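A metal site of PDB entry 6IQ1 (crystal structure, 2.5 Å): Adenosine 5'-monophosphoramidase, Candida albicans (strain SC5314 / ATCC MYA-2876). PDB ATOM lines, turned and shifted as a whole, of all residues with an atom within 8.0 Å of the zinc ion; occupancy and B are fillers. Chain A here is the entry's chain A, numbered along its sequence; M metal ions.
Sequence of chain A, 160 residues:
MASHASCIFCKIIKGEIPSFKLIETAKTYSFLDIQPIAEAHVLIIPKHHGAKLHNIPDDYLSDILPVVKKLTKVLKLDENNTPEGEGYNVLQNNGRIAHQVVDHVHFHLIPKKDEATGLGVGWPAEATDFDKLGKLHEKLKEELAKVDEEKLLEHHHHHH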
ATOM      1  N   SER A   6      22.586  -5.863 -15.850  1.00  0.00           N
ATOM      2  CA  SER A   6      22.783  -6.812 -16.959  1.00  0.00           C
ATOM      3  C   SER A   6      21.618  -7.786 -17.138  1.00  0.00           C
ATOM      4  O   SER A   6      21.563  -8.479 -18.164  1.00  0.00           O
ATOM      5  CB  SER A   6      24.070  -7.599 -16.751  1.00  0.00           C
ATOM      6  OG  SER A   6      23.856  -8.668 -15.851  1.00  0.00           O
ATOM      7  N   CYS A   7      20.704  -7.834 -16.171  1.00  0.00           N
ATOM      8  CA  CYS A   7      19.651  -8.857 -16.144  1.00  0.00           C
ATOM      9  C   CYS A   7      18.726  -8.707 -17.340  1.00  0.00           C
ATOM     10  O   CYS A   7      18.113  -7.657 -17.533  1.00  0.00           O
ATOM     11  CB  CYS A   7      18.844  -8.747 -14.850  1.00  0.00           C
ATOM     12  SG  CYS A   7      17.318  -9.774 -14.867  1.00  0.00           S
ATOM     13  N   ILE A   8      18.587  -9.780 -18.123  1.00  0.00           N
ATOM     14  CA  ILE A   8      17.778  -9.639 -19.335  1.00  0.00           C
ATOM     15  C   ILE A   8      16.307  -9.494 -19.004  1.00  0.00           C
ATOM     16  O   ILE A   8      15.552  -8.901 -19.787  1.00  0.00           O
ATOM     17  CB  ILE A   8      18.016 -10.804 -20.311  1.00  0.00           C
ATOM     18  CG1 ILE A   8      17.729 -12.122 -19.636  1.00  0.00           C
ATOM     19  CG2 ILE A   8      19.428 -10.773 -20.857  1.00  0.00           C
ATOM     20  CD1 ILE A   8      17.754 -13.264 -20.617  1.00  0.00           C
ATOM     21  N   PHE A   9      15.842 -10.033 -17.878  1.00  0.00           N
ATOM     22  CA  PHE A   9      14.406  -9.894 -17.622  1.00  0.00           C
ATOM     23  C   PHE A   9      14.068  -8.456 -17.223  1.00  0.00           C
ATOM     24  O   PHE A   9      13.073  -7.909 -17.721  1.00  0.00           O
ATOM     25  CB  PHE A   9      13.942 -10.913 -16.582  1.00  0.00           C
ATOM     26  CG  PHE A   9      13.776 -12.304 -17.135  1.00  0.00           C
ATOM     27  CD1 PHE A   9      14.096 -12.566 -18.465  1.00  0.00           C
ATOM     28  CD2 PHE A   9      13.337 -13.347 -16.353  1.00  0.00           C
ATOM     29  CE1 PHE A   9      13.962 -13.825 -18.986  1.00  0.00           C
ATOM     30  CE2 PHE A   9      13.187 -14.622 -16.873  1.00  0.00           C
ATOM     31  CZ  PHE A   9      13.507 -14.855 -18.197  1.00  0.00           C
ATOM     32  N   CYS A  10      14.901  -7.843 -16.385  1.00  0.00           N
ATOM     33  CA  CYS A  10      14.793  -6.418 -16.095  1.00  0.00           C
ATOM     34  C   CYS A  10      14.807  -5.574 -17.362  1.00  0.00           C
ATOM     35  O   CYS A  10      14.132  -4.544 -17.434  1.00  0.00           O
ATOM     36  CB  CYS A  10      15.932  -5.992 -15.155  1.00  0.00           C
ATOM     37  SG  CYS A  10      15.598  -6.439 -13.394  1.00  0.00           S
ATOM     38  N   LYS A  11      15.578  -6.007 -18.368  1.00  0.00           N
ATOM     39  CA  LYS A  11      15.610  -5.279 -19.629  1.00  0.00           C
ATOM     40  C   LYS A  11      14.315  -5.471 -20.400  1.00  0.00           C
ATOM     41  O   LYS A  11      13.852  -4.553 -21.102  1.00  0.00           O
ATOM     42  CB  LYS A  11      16.806  -5.712 -20.471  1.00  0.00           C
ATOM     43  CG  LYS A  11      18.120  -5.198 -19.984  1.00  0.00           C
ATOM     44  CD  LYS A  11      19.242  -5.660 -20.868  1.00  0.00           C
ATOM     45  CE  LYS A  11      20.575  -5.078 -20.423  1.00  0.00           C
ATOM     46  NZ  LYS A  11      21.651  -6.090 -20.648  1.00  0.00           N
ATOM     47  N   ILE A  12      13.742  -6.666 -20.308  1.00  0.00           N
ATOM     48  CA  ILE A  12      12.425  -6.897 -20.900  1.00  0.00           C
ATOM     49  C   ILE A  12      11.402  -5.966 -20.262  1.00  0.00           C
ATOM     50  O   ILE A  12      10.622  -5.305 -20.956  1.00  0.00           O
ATOM     51  CB  ILE A  12      12.019  -8.366 -20.760  1.00  0.00           C
ATOM     52  CG1 ILE A  12      12.785  -9.207 -21.783  1.00  0.00           C
ATOM     53  CG2 ILE A  12      10.502  -8.509 -20.916  1.00  0.00           C
ATOM     54  CD1 ILE A  12      12.585 -10.712 -21.646  1.00  0.00           C
ATOM     55  N   ILE A  13      11.416  -5.891 -18.929  1.00  0.00           N
ATOM     56  CA  ILE A  13      10.478  -5.031 -18.217  1.00  0.00           C
ATOM     57  C   ILE A  13      10.654  -3.579 -18.652  1.00  0.00           C
ATOM     58  O   ILE A  13       9.665  -2.877 -18.891  1.00  0.00           O
ATOM     59  CB  ILE A  13      10.661  -5.205 -16.706  1.00  0.00           C
ATOM     60  CG1 ILE A  13      10.216  -6.588 -16.295  1.00  0.00           C
ATOM     61  CG2 ILE A  13       9.816  -4.237 -15.945  1.00  0.00           C
ATOM     62  CD1 ILE A  13      10.788  -6.966 -14.963  1.00  0.00           C
ATOM     63  N   ILE A  45       6.838 -12.903 -14.330  1.00  0.00           N
ATOM     64  CA  ILE A  45       7.912 -12.459 -13.450  1.00  0.00           C
ATOM     65  C   ILE A  45       7.450 -11.282 -12.597  1.00  0.00           C
ATOM     66  O   ILE A  45       6.628 -10.464 -13.052  1.00  0.00           O
ATOM     67  CB  ILE A  45       9.189 -12.124 -14.255  1.00  0.00           C
ATOM     68  CG1 ILE A  45       9.111 -10.739 -14.885  1.00  0.00           C
ATOM     69  CG2 ILE A  45       9.372 -13.112 -15.386  1.00  0.00           C
ATOM     70  CD1 ILE A  45      10.311 -10.379 -15.749  1.00  0.00           C
ATOM     71  N   PRO A  46       7.914 -11.172 -11.363  1.00  0.00           N
ATOM     72  CA  PRO A  46       7.663  -9.940 -10.599  1.00  0.00           C
ATOM     73  C   PRO A  46       8.587  -8.854 -11.108  1.00  0.00           C
ATOM     74  O   PRO A  46       9.668  -9.106 -11.665  1.00  0.00           O
ATOM     75  CB  PRO A  46       8.007 -10.346  -9.167  1.00  0.00           C
ATOM     76  CG  PRO A  46       9.084 -11.388  -9.351  1.00  0.00           C
ATOM     77  CD  PRO A  46       8.750 -12.131 -10.617  1.00  0.00           C
ATOM     78  N   LYS A  47       8.136  -7.605 -10.955  1.00  0.00           N
ATOM     79  CA  LYS A  47       8.977  -6.527 -11.443  1.00  0.00           C
ATOM     80  C   LYS A  47      10.135  -6.241 -10.519  1.00  0.00           C
ATOM     81  O   LYS A  47      11.146  -5.668 -10.955  1.00  0.00           O
ATOM     82  CB  LYS A  47       8.144  -5.271 -11.679  1.00  0.00           C
ATOM     83  CG  LYS A  47       7.283  -5.403 -12.907  1.00  0.00           C
ATOM     84  CD  LYS A  47       6.439  -4.185 -13.105  1.00  0.00           C
ATOM     85  CE  LYS A  47       5.524  -4.345 -14.273  1.00  0.00           C
ATOM     86  NZ  LYS A  47       4.738  -3.113 -14.428  1.00  0.00           N
ATOM     87  N   HIS A  48      10.045  -6.692  -9.279  1.00  0.00           N
ATOM     88  CA  HIS A  48      11.129  -6.605  -8.316  1.00  0.00           C
ATOM     89  C   HIS A  48      12.165  -7.668  -8.644  1.00  0.00           C
ATOM     90  O   HIS A  48      11.868  -8.872  -8.574  1.00  0.00           O
ATOM     91  CB  HIS A  48      10.599  -6.795  -6.906  1.00  0.00           C
ATOM     92  CG  HIS A  48      11.646  -6.725  -5.837  1.00  0.00           C
ATOM     93  ND1 HIS A  48      12.519  -7.759  -5.578  1.00  0.00           N
ATOM     94  CD2 HIS A  48      11.954  -5.732  -4.957  1.00  0.00           C
ATOM     95  CE1 HIS A  48      13.326  -7.414  -4.581  1.00  0.00           C
ATOM     96  NE2 HIS A  48      13.000  -6.191  -4.187  1.00  0.00           N
ATOM     97  N   HIS A  49      13.371  -7.230  -8.994  1.00  0.00           N
ATOM     98  CA  HIS A  49      14.454  -8.146  -9.321  1.00  0.00           C
ATOM     99  C   HIS A  49      14.947  -8.858  -8.063  1.00  0.00           C
ATOM    100  O   HIS A  49      15.445  -8.233  -7.129  1.00  0.00           O
ATOM    101  CB  HIS A  49      15.617  -7.395  -9.991  1.00  0.00           C
ATOM    102  CG  HIS A  49      16.857  -8.217 -10.097  1.00  0.00           C
ATOM    103  ND1 HIS A  49      17.146  -8.983 -11.206  1.00  0.00           N
ATOM    104  CD2 HIS A  49      17.862  -8.433  -9.218  1.00  0.00           C
ATOM    105  CE1 HIS A  49      18.286  -9.626 -11.014  1.00  0.00           C
ATOM    106  NE2 HIS A  49      18.741  -9.306  -9.813  1.00  0.00           N
ATOM    107  N   GLY A  50      14.804 -10.191  -8.044  1.00  0.00           N
ATOM    108  CA  GLY A  50      15.419 -11.043  -7.055  1.00  0.00           C
ATOM    109  C   GLY A  50      15.711 -12.369  -7.712  1.00  0.00           C
ATOM    110  O   GLY A  50      14.902 -12.821  -8.519  1.00  0.00           O
ATOM    111  N   ALA A  51      16.836 -13.004  -7.389  1.00  0.00           N
ATOM    112  CA  ALA A  51      17.230 -14.210  -8.118  1.00  0.00           C
ATOM    113  C   ALA A  51      16.364 -15.416  -7.749  1.00  0.00           C
ATOM    114  O   ALA A  51      15.954 -16.181  -8.623  1.00  0.00           O
ATOM    115  CB  ALA A  51      18.702 -14.528  -7.876  1.00  0.00           C
ATOM    116  N   VAL A 102      18.345 -17.898 -15.944  1.00  0.00           N
ATOM    117  CA  VAL A 102      18.203 -16.450 -15.800  1.00  0.00           C
ATOM    118  C   VAL A 102      17.928 -16.146 -14.327  1.00  0.00           C
ATOM    119  O   VAL A 102      16.942 -16.623 -13.761  1.00  0.00           O
ATOM    120  CB  VAL A 102      17.094 -15.907 -16.699  1.00  0.00           C
ATOM    121  CG1 VAL A 102      16.896 -14.391 -16.474  1.00  0.00           C
ATOM    122  CG2 VAL A 102      17.426 -16.194 -18.175  1.00  0.00           C
ATOM    123  N   ASP A 103      18.810 -15.369 -13.710  1.00  0.00           N
ATOM    124  CA  ASP A 103      18.829 -15.189 -12.253  1.00  0.00           C
ATOM    125  C   ASP A 103      17.878 -14.099 -11.770  1.00  0.00           C
ATOM    126  O   ASP A 103      18.233 -13.171 -11.055  1.00  0.00           O
ATOM    127  CB  ASP A 103      20.263 -14.938 -11.802  1.00  0.00           C
ATOM    128  CG  ASP A 103      21.112 -16.217 -11.859  1.00  0.00           C
ATOM    129  OD1 ASP A 103      20.527 -17.299 -11.589  1.00  0.00           O
ATOM    130  OD2 ASP A 103      22.318 -16.151 -12.195  1.00  0.00           O
ATOM    131  N   HIS A 104      16.624 -14.258 -12.188  1.00  0.00           N
ATOM    132  CA  HIS A 104      15.515 -13.373 -11.851  1.00  0.00           C
ATOM    133  C   HIS A 104      14.281 -14.271 -11.787  1.00  0.00           C
ATOM    134  O   HIS A 104      14.044 -15.024 -12.728  1.00  0.00           O
ATOM    135  CB  HIS A 104      15.360 -12.249 -12.893  1.00  0.00           C
ATOM    136  CG  HIS A 104      14.255 -11.281 -12.608  1.00  0.00           C
ATOM    137  ND1 HIS A 104      14.400  -9.921 -12.752  1.00  0.00           N
ATOM    138  CD2 HIS A 104      12.955 -11.475 -12.261  1.00  0.00           C
ATOM    139  CE1 HIS A 104      13.276  -9.313 -12.476  1.00  0.00           C
ATOM    140  NE2 HIS A 104      12.374 -10.224 -12.170  1.00  0.00           N
ATOM    141  N   VAL A 105      13.540 -14.204 -10.693  1.00  0.00           N
ATOM    142  CA  VAL A 105      12.494 -15.197 -10.463  1.00  0.00           C
ATOM    143  C   VAL A 105      11.545 -15.197 -11.640  1.00  0.00           C
ATOM    144  O   VAL A 105      11.100 -14.132 -12.083  1.00  0.00           O
ATOM    145  CB  VAL A 105      11.760 -14.895  -9.146  1.00  0.00           C
ATOM    146  CG1 VAL A 105      10.378 -15.573  -9.117  1.00  0.00           C
ATOM    147  CG2 VAL A 105      12.595 -15.340  -8.004  1.00  0.00           C
HETATM  148 ZN    ZN M   1      16.135  -8.732 -13.121  1.00  0.00          ZN
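The backbone carbonyl oxygen of Pro 46 is in hydrogen-bond range of a ring nitrogen (NE2) of His 104 (3.0 Å).
The backbone NH (N) of Phe 9 sits close to the side-chain sulfur (SG) of Cys 7 (3.4 Å).
Four residues have an atom within 4 Å of the zinc ion: Cys 7, Cys 10, His 49 and His 104.
The zinc ion is bound by a ring nitrogen (ND1) of His 104, a ring nitrogen (ND1) of His 49, the side-chain sulfur of Cys 7 and the side-chain sulfur of Cys 10.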
